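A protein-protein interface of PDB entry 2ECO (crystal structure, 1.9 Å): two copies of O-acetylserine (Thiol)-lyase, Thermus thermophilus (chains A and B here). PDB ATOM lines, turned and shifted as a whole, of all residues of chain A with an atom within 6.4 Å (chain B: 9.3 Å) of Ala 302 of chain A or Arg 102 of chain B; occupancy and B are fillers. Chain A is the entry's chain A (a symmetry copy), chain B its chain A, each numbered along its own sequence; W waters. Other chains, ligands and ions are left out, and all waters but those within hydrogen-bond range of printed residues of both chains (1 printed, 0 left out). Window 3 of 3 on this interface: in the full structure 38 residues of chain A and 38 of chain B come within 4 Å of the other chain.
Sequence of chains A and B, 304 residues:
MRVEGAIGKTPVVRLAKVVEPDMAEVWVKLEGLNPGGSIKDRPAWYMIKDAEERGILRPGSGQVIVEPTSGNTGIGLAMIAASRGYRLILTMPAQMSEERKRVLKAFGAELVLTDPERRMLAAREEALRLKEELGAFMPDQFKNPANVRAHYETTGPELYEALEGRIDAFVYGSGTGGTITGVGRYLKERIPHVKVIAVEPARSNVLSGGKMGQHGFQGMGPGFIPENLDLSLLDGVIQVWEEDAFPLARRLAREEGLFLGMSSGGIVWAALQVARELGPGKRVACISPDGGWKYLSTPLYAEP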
ATOM      1  N   PHE A 259      20.478   3.737 -23.198  1.00  0.00           N
ATOM      2  CA  PHE A 259      19.966   2.437 -22.765  1.00  0.00           C
ATOM      3  C   PHE A 259      19.095   1.895 -23.896  1.00  0.00           C
ATOM      4  O   PHE A 259      17.891   2.149 -23.943  1.00  0.00           O
ATOM      5  CB  PHE A 259      19.146   2.650 -21.485  1.00  0.00           C
ATOM      6  CG  PHE A 259      18.552   1.397 -20.908  1.00  0.00           C
ATOM      7  CD1 PHE A 259      19.349   0.295 -20.623  1.00  0.00           C
ATOM      8  CD2 PHE A 259      17.197   1.342 -20.601  1.00  0.00           C
ATOM      9  CE1 PHE A 259      18.804  -0.848 -20.035  1.00  0.00           C
ATOM     10  CE2 PHE A 259      16.640   0.203 -20.012  1.00  0.00           C
ATOM     11  CZ  PHE A 259      17.446  -0.892 -19.728  1.00  0.00           C
ATOM     12  N   TYR A 295      13.942  -5.376 -22.150  1.00  0.00           N
ATOM     13  CA  TYR A 295      14.898  -6.475 -22.077  1.00  0.00           C
ATOM     14  C   TYR A 295      15.701  -6.636 -20.788  1.00  0.00           C
ATOM     15  O   TYR A 295      16.802  -7.181 -20.800  1.00  0.00           O
ATOM     16  CB  TYR A 295      15.850  -6.376 -23.272  1.00  0.00           C
ATOM     17  CG  TYR A 295      15.129  -6.086 -24.574  1.00  0.00           C
ATOM     18  CD1 TYR A 295      15.050  -4.786 -25.079  1.00  0.00           C
ATOM     19  CD2 TYR A 295      14.496  -7.108 -25.283  1.00  0.00           C
ATOM     20  CE1 TYR A 295      14.356  -4.510 -26.267  1.00  0.00           C
ATOM     21  CE2 TYR A 295      13.798  -6.845 -26.466  1.00  0.00           C
ATOM     22  CZ  TYR A 295      13.733  -5.548 -26.950  1.00  0.00           C
ATOM     23  OH  TYR A 295      13.048  -5.297 -28.118  1.00  0.00           O
ATOM     24  N   LEU A 296      15.145  -6.186 -19.673  1.00  0.00           N
ATOM     25  CA  LEU A 296      15.840  -6.301 -18.398  1.00  0.00           C
ATOM     26  C   LEU A 296      15.965  -7.755 -17.943  1.00  0.00           C
ATOM     27  O   LEU A 296      16.833  -8.088 -17.134  1.00  0.00           O
ATOM     28  CB  LEU A 296      15.111  -5.481 -17.334  1.00  0.00           C
ATOM     29  CG  LEU A 296      15.102  -3.966 -17.555  1.00  0.00           C
ATOM     30  CD1 LEU A 296      14.218  -3.310 -16.513  1.00  0.00           C
ATOM     31  CD2 LEU A 296      16.521  -3.429 -17.478  1.00  0.00           C
ATOM     32  N   SER A 297      15.105  -8.622 -18.469  1.00  0.00           N
ATOM     33  CA  SER A 297      15.127 -10.031 -18.095  1.00  0.00           C
ATOM     34  C   SER A 297      15.895 -10.895 -19.089  1.00  0.00           C
ATOM     35  O   SER A 297      15.791 -12.122 -19.061  1.00  0.00           O
ATOM     36  CB  SER A 297      13.698 -10.562 -17.957  1.00  0.00           C
ATOM     37  OG  SER A 297      12.988  -9.853 -16.955  1.00  0.00           O
ATOM     38  N   THR A 298      16.663 -10.255 -19.964  1.00  0.00           N
ATOM     39  CA  THR A 298      17.444 -10.977 -20.959  1.00  0.00           C
ATOM     40  C   THR A 298      18.918 -10.914 -20.578  1.00  0.00           C
ATOM     41  O   THR A 298      19.307 -10.123 -19.722  1.00  0.00           O
ATOM     42  CB  THR A 298      17.280 -10.355 -22.361  1.00  0.00           C
ATOM     43  OG1 THR A 298      17.894  -9.059 -22.382  1.00  0.00           O
ATOM     44  CG2 THR A 298      15.805 -10.219 -22.712  1.00  0.00           C
ATOM     45  N   PRO A 299      19.756 -11.749 -21.210  1.00  0.00           N
ATOM     46  CA  PRO A 299      21.190 -11.754 -20.909  1.00  0.00           C
ATOM     47  C   PRO A 299      21.889 -10.440 -21.251  1.00  0.00           C
ATOM     48  O   PRO A 299      23.050 -10.236 -20.898  1.00  0.00           O
ATOM     49  CB  PRO A 299      21.711 -12.930 -21.733  1.00  0.00           C
ATOM     50  CG  PRO A 299      20.759 -12.988 -22.885  1.00  0.00           C
ATOM     51  CD  PRO A 299      19.432 -12.780 -22.211  1.00  0.00           C
ATOM     52  N   LEU A 300      21.182  -9.546 -21.937  1.00  0.00           N
ATOM     53  CA  LEU A 300      21.766  -8.259 -22.299  1.00  0.00           C
ATOM     54  C   LEU A 300      21.989  -7.409 -21.053  1.00  0.00           C
ATOM     55  O   LEU A 300      23.056  -6.827 -20.878  1.00  0.00           O
ATOM     56  CB  LEU A 300      20.855  -7.499 -23.271  1.00  0.00           C
ATOM     57  CG  LEU A 300      21.324  -6.092 -23.659  1.00  0.00           C
ATOM     58  CD1 LEU A 300      22.703  -6.168 -24.298  1.00  0.00           C
ATOM     59  CD2 LEU A 300      20.328  -5.454 -24.618  1.00  0.00           C
ATOM     60  N   TYR A 301      20.981  -7.356 -20.185  1.00  0.00           N
ATOM     61  CA  TYR A 301      21.060  -6.554 -18.965  1.00  0.00           C
ATOM     62  C   TYR A 301      20.828  -7.320 -17.663  1.00  0.00           C
ATOM     63  O   TYR A 301      20.926  -6.738 -16.582  1.00  0.00           O
ATOM     64  CB  TYR A 301      20.055  -5.399 -19.039  1.00  0.00           C
ATOM     65  CG  TYR A 301      20.317  -4.418 -20.161  1.00  0.00           C
ATOM     66  CD1 TYR A 301      19.378  -4.218 -21.174  1.00  0.00           C
ATOM     67  CD2 TYR A 301      21.494  -3.673 -20.198  1.00  0.00           C
ATOM     68  CE1 TYR A 301      19.607  -3.295 -22.197  1.00  0.00           C
ATOM     69  CE2 TYR A 301      21.733  -2.748 -21.215  1.00  0.00           C
ATOM     70  CZ  TYR A 301      20.786  -2.564 -22.209  1.00  0.00           C
ATOM     71  OH  TYR A 301      21.022  -1.648 -23.211  1.00  0.00           O
ATOM     72  N   ALA A 302      20.516  -8.609 -17.753  1.00  0.00           N
ATOM     73  CA  ALA A 302      20.272  -9.403 -16.551  1.00  0.00           C
ATOM     74  C   ALA A 302      21.572  -9.794 -15.855  1.00  0.00           C
ATOM     75  O   ALA A 302      22.652  -9.590 -16.451  1.00  0.00           O
ATOM     76  CB  ALA A 302      19.469 -10.653 -16.899  1.00  0.00           C
ATOM     77  N   SER B  70      15.974   5.612  -5.760  1.00  0.00           N
ATOM     78  CA  SER B  70      16.016   4.457  -6.647  1.00  0.00           C
ATOM     79  C   SER B  70      14.880   4.619  -7.656  1.00  0.00           C
ATOM     80  O   SER B  70      14.641   3.743  -8.493  1.00  0.00           O
ATOM     81  CB  SER B  70      15.812   3.176  -5.845  1.00  0.00           C
ATOM     82  OG  SER B  70      14.581   3.228  -5.152  1.00  0.00           O
ATOM     83  N   ILE B  75      17.162   7.138 -12.113  1.00  0.00           N
ATOM     84  CA  ILE B  75      17.348   6.764 -13.513  1.00  0.00           C
ATOM     85  C   ILE B  75      17.805   7.973 -14.329  1.00  0.00           C
ATOM     86  O   ILE B  75      18.733   7.879 -15.129  1.00  0.00           O
ATOM     87  CB  ILE B  75      16.035   6.217 -14.122  1.00  0.00           C
ATOM     88  CG1 ILE B  75      15.606   4.953 -13.374  1.00  0.00           C
ATOM     89  CG2 ILE B  75      16.231   5.929 -15.602  1.00  0.00           C
ATOM     90  CD1 ILE B  75      14.243   4.410 -13.808  1.00  0.00           C
ATOM     91  N   ALA B  78      21.343   8.799 -13.403  1.00  0.00           N
ATOM     92  CA  ALA B  78      22.245   7.779 -13.919  1.00  0.00           C
ATOM     93  C   ALA B  78      22.525   8.029 -15.397  1.00  0.00           C
ATOM     94  O   ALA B  78      23.664   7.938 -15.853  1.00  0.00           O
ATOM     95  CB  ALA B  78      21.637   6.388 -13.716  1.00  0.00           C
ATOM     96  N   MET B  92      19.699   3.374  -1.413  1.00  0.00           N
ATOM     97  CA  MET B  92      18.309   2.930  -1.403  1.00  0.00           C
ATOM     98  C   MET B  92      18.124   1.704  -0.520  1.00  0.00           C
ATOM     99  O   MET B  92      19.061   0.933  -0.313  1.00  0.00           O
ATOM    100  CB  MET B  92      17.896   2.569  -2.828  1.00  0.00           C
ATOM    101  CG  MET B  92      18.753   1.437  -3.398  1.00  0.00           C
ATOM    102  SD  MET B  92      18.677   1.258  -5.188  1.00  0.00           S
ATOM    103  CE  MET B  92      19.534   2.755  -5.701  1.00  0.00           C
ATOM    104  N   MET B  96      14.914  -3.220  -2.578  1.00  0.00           N
ATOM    105  CA  MET B  96      14.692  -2.765  -3.950  1.00  0.00           C
ATOM    106  C   MET B  96      14.523  -3.928  -4.925  1.00  0.00           C
ATOM    107  O   MET B  96      15.177  -4.964  -4.790  1.00  0.00           O
ATOM    108  CB  MET B  96      15.852  -1.875  -4.398  1.00  0.00           C
ATOM    109  N   SER B  97      13.649  -3.753  -5.911  1.00  0.00           N
ATOM    110  CA  SER B  97      13.402  -4.795  -6.901  1.00  0.00           C
ATOM    111  C   SER B  97      14.597  -4.968  -7.835  1.00  0.00           C
ATOM    112  O   SER B  97      15.275  -3.998  -8.182  1.00  0.00           O
ATOM    113  CB  SER B  97      12.148  -4.468  -7.721  1.00  0.00           C
ATOM    114  OG  SER B  97      12.339  -3.326  -8.540  1.00  0.00           O
ATOM    115  N   GLU B  98      14.848  -6.209  -8.238  1.00  0.00           N
ATOM    116  CA  GLU B  98      15.958  -6.518  -9.129  1.00  0.00           C
ATOM    117  C   GLU B  98      15.825  -5.780 -10.452  1.00  0.00           C
ATOM    118  O   GLU B  98      16.819  -5.380 -11.053  1.00  0.00           O
ATOM    119  CB  GLU B  98      16.022  -8.024  -9.390  1.00  0.00           C
ATOM    120  CG  GLU B  98      16.333  -8.854  -8.156  1.00  0.00           C
ATOM    121  CD  GLU B  98      17.675  -8.499  -7.547  1.00  0.00           C
ATOM    122  OE1 GLU B  98      18.686  -8.542  -8.280  1.00  0.00           O
ATOM    123  OE2 GLU B  98      17.716  -8.180  -6.341  1.00  0.00           O
ATOM    124  N   GLU B  99      14.586  -5.606 -10.900  1.00  0.00           N
ATOM    125  CA  GLU B  99      14.315  -4.918 -12.153  1.00  0.00           C
ATOM    126  C   GLU B  99      14.903  -3.509 -12.133  1.00  0.00           C
ATOM    127  O   GLU B  99      15.678  -3.137 -13.017  1.00  0.00           O
ATOM    128  CB  GLU B  99      12.805  -4.842 -12.393  1.00  0.00           C
ATOM    129  CG  GLU B  99      12.423  -4.558 -13.836  1.00  0.00           C
ATOM    130  CD  GLU B  99      10.923  -4.425 -14.028  1.00  0.00           C
ATOM    131  OE1 GLU B  99      10.174  -5.224 -13.427  1.00  0.00           O
ATOM    132  OE2 GLU B  99      10.497  -3.530 -14.788  1.00  0.00           O
ATOM    133  N   ARG B 100      14.530  -2.730 -11.122  1.00  0.00           N
ATOM    134  CA  ARG B 100      15.018  -1.362 -10.992  1.00  0.00           C
ATOM    135  C   ARG B 100      16.535  -1.329 -10.832  1.00  0.00           C
ATOM    136  O   ARG B 100      17.219  -0.530 -11.473  1.00  0.00           O
ATOM    137  CB  ARG B 100      14.351  -0.673  -9.798  1.00  0.00           C
ATOM    138  CG  ARG B 100      14.711   0.805  -9.646  1.00  0.00           C
ATOM    139  CD  ARG B 100      14.440   1.585 -10.932  1.00  0.00           C
ATOM    140  NE  ARG B 100      13.045   1.485 -11.363  1.00  0.00           N
ATOM    141  CZ  ARG B 100      12.027   2.104 -10.769  1.00  0.00           C
ATOM    142  NH1 ARG B 100      12.242   2.879  -9.715  1.00  0.00           N
ATOM    143  NH2 ARG B 100      10.791   1.944 -11.228  1.00  0.00           N
ATOM    144  N   LYS B 101      17.060  -2.199  -9.977  1.00  0.00           N
ATOM    145  CA  LYS B 101      18.498  -2.259  -9.763  1.00  0.00           C
ATOM    146  C   LYS B 101      19.215  -2.508 -11.091  1.00  0.00           C
ATOM    147  O   LYS B 101      20.274  -1.937 -11.350  1.00  0.00           O
ATOM    148  CB  LYS B 101      18.830  -3.361  -8.750  1.00  0.00           C
ATOM    149  CG  LYS B 101      18.398  -3.021  -7.322  1.00  0.00           C
ATOM    150  CD  LYS B 101      18.262  -4.261  -6.437  1.00  0.00           C
ATOM    151  CE  LYS B 101      19.569  -5.026  -6.312  1.00  0.00           C
ATOM    152  NZ  LYS B 101      19.440  -6.192  -5.387  1.00  0.00           N
ATOM    153  N   ARG B 102      18.629  -3.349 -11.939  1.00  0.00           N
ATOM    154  CA  ARG B 102      19.231  -3.650 -13.234  1.00  0.00           C
ATOM    155  C   ARG B 102      19.298  -2.428 -14.145  1.00  0.00           C
ATOM    156  O   ARG B 102      20.288  -2.227 -14.848  1.00  0.00           O
ATOM    157  CB  ARG B 102      18.458  -4.768 -13.934  1.00  0.00           C
ATOM    158  CG  ARG B 102      18.752  -6.147 -13.376  1.00  0.00           C
ATOM    159  CD  ARG B 102      17.801  -7.184 -13.938  1.00  0.00           C
ATOM    160  NE  ARG B 102      18.190  -8.534 -13.547  1.00  0.00           N
ATOM    161  CZ  ARG B 102      17.445  -9.613 -13.759  1.00  0.00           C
ATOM    162  NH1 ARG B 102      16.266  -9.499 -14.358  1.00  0.00           N
ATOM    163  NH2 ARG B 102      17.881 -10.806 -13.376  1.00  0.00           N
ATOM    164  N   VAL B 103      18.243  -1.620 -14.138  1.00  0.00           N
ATOM    165  CA  VAL B 103      18.208  -0.421 -14.967  1.00  0.00           C
ATOM    166  C   VAL B 103      19.286   0.555 -14.505  1.00  0.00           C
ATOM    167  O   VAL B 103      20.055   1.072 -15.315  1.00  0.00           O
ATOM    168  CB  VAL B 103      16.837   0.279 -14.886  1.00  0.00           C
ATOM    169  CG1 VAL B 103      16.879   1.602 -15.639  1.00  0.00           C
ATOM    170  CG2 VAL B 103      15.761  -0.617 -15.477  1.00  0.00           C
ATOM    171  N   LEU B 104      19.344   0.797 -13.199  1.00  0.00           N
ATOM    172  CA  LEU B 104      20.334   1.716 -12.647  1.00  0.00           C
ATOM    173  C   LEU B 104      21.757   1.260 -12.950  1.00  0.00           C
ATOM    174  O   LEU B 104      22.589   2.055 -13.386  1.00  0.00           O
ATOM    175  CB  LEU B 104      20.125   1.864 -11.137  1.00  0.00           C
ATOM    176  CG  LEU B 104      18.760   2.438 -10.734  1.00  0.00           C
ATOM    177  CD1 LEU B 104      18.612   2.406  -9.220  1.00  0.00           C
ATOM    178  CD2 LEU B 104      18.618   3.869 -11.261  1.00  0.00           C
ATOM    179  N   LYS B 105      22.038  -0.024 -12.737  1.00  0.00           N
ATOM    180  CA  LYS B 105      23.371  -0.557 -13.000  1.00  0.00           C
ATOM    181  C   LYS B 105      23.709  -0.534 -14.488  1.00  0.00           C
ATOM    182  O   LYS B 105      24.878  -0.469 -14.862  1.00  0.00           O
ATOM    183  CB  LYS B 105      23.496  -1.987 -12.468  1.00  0.00           C
ATOM    184  CG  LYS B 105      23.473  -2.087 -10.948  1.00  0.00           C
ATOM    185  CD  LYS B 105      23.676  -3.526 -10.498  1.00  0.00           C
ATOM    186  CE  LYS B 105      23.714  -3.631  -8.986  1.00  0.00           C
ATOM    187  NZ  LYS B 105      24.795  -2.779  -8.417  1.00  0.00           N
ATOM    188  N   ALA B 106      22.685  -0.598 -15.333  1.00  0.00           N
ATOM    189  CA  ALA B 106      22.903  -0.565 -16.775  1.00  0.00           C
ATOM    190  C   ALA B 106      23.565   0.766 -17.127  1.00  0.00           C
ATOM    191  O   ALA B 106      24.451   0.829 -17.982  1.00  0.00           O
ATOM    192  CB  ALA B 106      21.576  -0.703 -17.511  1.00  0.00           C
ATOM    193  N   PHE B 107      23.130   1.826 -16.451  1.00  0.00           N
ATOM    194  CA  PHE B 107      23.674   3.161 -16.673  1.00  0.00           C
ATOM    195  C   PHE B 107      24.999   3.375 -15.949  1.00  0.00           C
ATOM    196  O   PHE B 107      25.582   4.459 -16.014  1.00  0.00           O
ATOM    197  CB  PHE B 107      22.675   4.227 -16.221  1.00  0.00           C
ATOM    198  CG  PHE B 107      21.523   4.428 -17.166  1.00  0.00           C
ATOM    199  CD1 PHE B 107      20.241   4.011 -16.822  1.00  0.00           C
ATOM    200  CD2 PHE B 107      21.719   5.049 -18.397  1.00  0.00           C
ATOM    201  CE1 PHE B 107      19.169   4.215 -17.686  1.00  0.00           C
ATOM    202  CE2 PHE B 107      20.652   5.257 -19.269  1.00  0.00           C
ATOM    203  CZ  PHE B 107      19.375   4.840 -18.912  1.00  0.00           C
ATOM    204  N   GLY B 108      25.473   2.348 -15.255  1.00  0.00           N
ATOM    205  CA  GLY B 108      26.738   2.465 -14.553  1.00  0.00           C
ATOM    206  C   GLY B 108      26.676   3.090 -13.168  1.00  0.00           C
ATOM    207  O   GLY B 108      27.711   3.416 -12.587  1.00  0.00           O
ATOM    208  N   ALA B 109      25.474   3.268 -12.636  1.00  0.00           N
ATOM    209  CA  ALA B 109      25.332   3.837 -11.303  1.00  0.00           C
ATOM    210  C   ALA B 109      25.775   2.801 -10.271  1.00  0.00           C
ATOM    211  O   ALA B 109      25.570   1.601 -10.458  1.00  0.00           O
ATOM    212  CB  ALA B 109      23.884   4.229 -11.053  1.00  0.00           C
ATOM    213  N   LEU B 111      25.278   1.257  -6.638  1.00  0.00           N
ATOM    214  CA  LEU B 111      24.182   1.203  -5.680  1.00  0.00           C
ATOM    215  C   LEU B 111      24.640   0.808  -4.282  1.00  0.00           C
ATOM    216  O   LEU B 111      25.458  -0.097  -4.116  1.00  0.00           O
ATOM    217  CB  LEU B 111      23.118   0.205  -6.153  1.00  0.00           C
ATOM    218  CG  LEU B 111      22.707   0.254  -7.627  1.00  0.00           C
ATOM    219  CD1 LEU B 111      21.636  -0.805  -7.891  1.00  0.00           C
ATOM    220  CD2 LEU B 111      22.187   1.642  -7.978  1.00  0.00           C
HETATM  221  O   HOH W   1      22.026  -4.295 -15.774  1.00  0.00           O
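Printed residues of chain B within 4 Å of Leu 296 of chain A: Glu 99 (3.5 Å), Arg 102 (3.2 Å) and Val 103 (3.3 Å). Leu 300 of chain A touches none of the printed residues of chain B. Of the printed residues of chain B, Tyr 301 of chain A touches Arg 102. Of chain B, only Arg 102 (3.8 Å) comes within 4 Å of Ala 302 of chain A. Of the printed residues of chain A, Glu 99 of chain B touches Leu 296 (3.5 Å). Arg 102 of chain B touches four residues of chain A. Of the printed residues of chain A, Ala 106 of chain B touches Phe 259 (3.8 Å). Of the printed residues of chain A, Phe 107 of chain B touches Phe 259.
No position is printed for both chains. Of the 8 pairs that touch across the chains among the printed residues, none has its exchanged pair printed and touching as well.
Water W1 lies within hydrogen-bond range of O of Tyr 301 of chain A and O of Arg 102 of chain B.
Printed residues of chain B that touch a printed residue of chain A: Glu 99, Arg 102, Val 103, Ala 106 and Phe 107. Hydrophobic or aromatic side chains of chain B that line the printed part of chain A: Val 103, Ala 106 and Phe 107. Of the 9 printed residues of chain A, 5 touch a printed residue of chain B. Hydrophobic or aromatic side chains of chain A that line the printed part of chain B: Phe 259, Leu 296 and Ala 302. Among the printed residues, no Asp or Glu carboxylate lies within 4 Å of a Lys or Arg side-chain nitrogen of the other chain.
Among the printed residues, pairs that only touch across the chains: Leu 296 of chain A with Val 103 of chain B, Phe 259 of chain A with Phe 107 of chain B, Leu 296 of chain A with Glu 99 of chain B, Phe 259 of chain A with Ala 106 of chain B, Ala 302 of chain A with Arg 102 of chain B, Tyr 301 of chain A with Arg 102 of chain B and Ser 297 of chain A with Arg 102 of chain B.
NH1 of Arg 102 of chain B lies within hydrogen-bond range of O of Leu 296 of chain A (3.2 Å).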
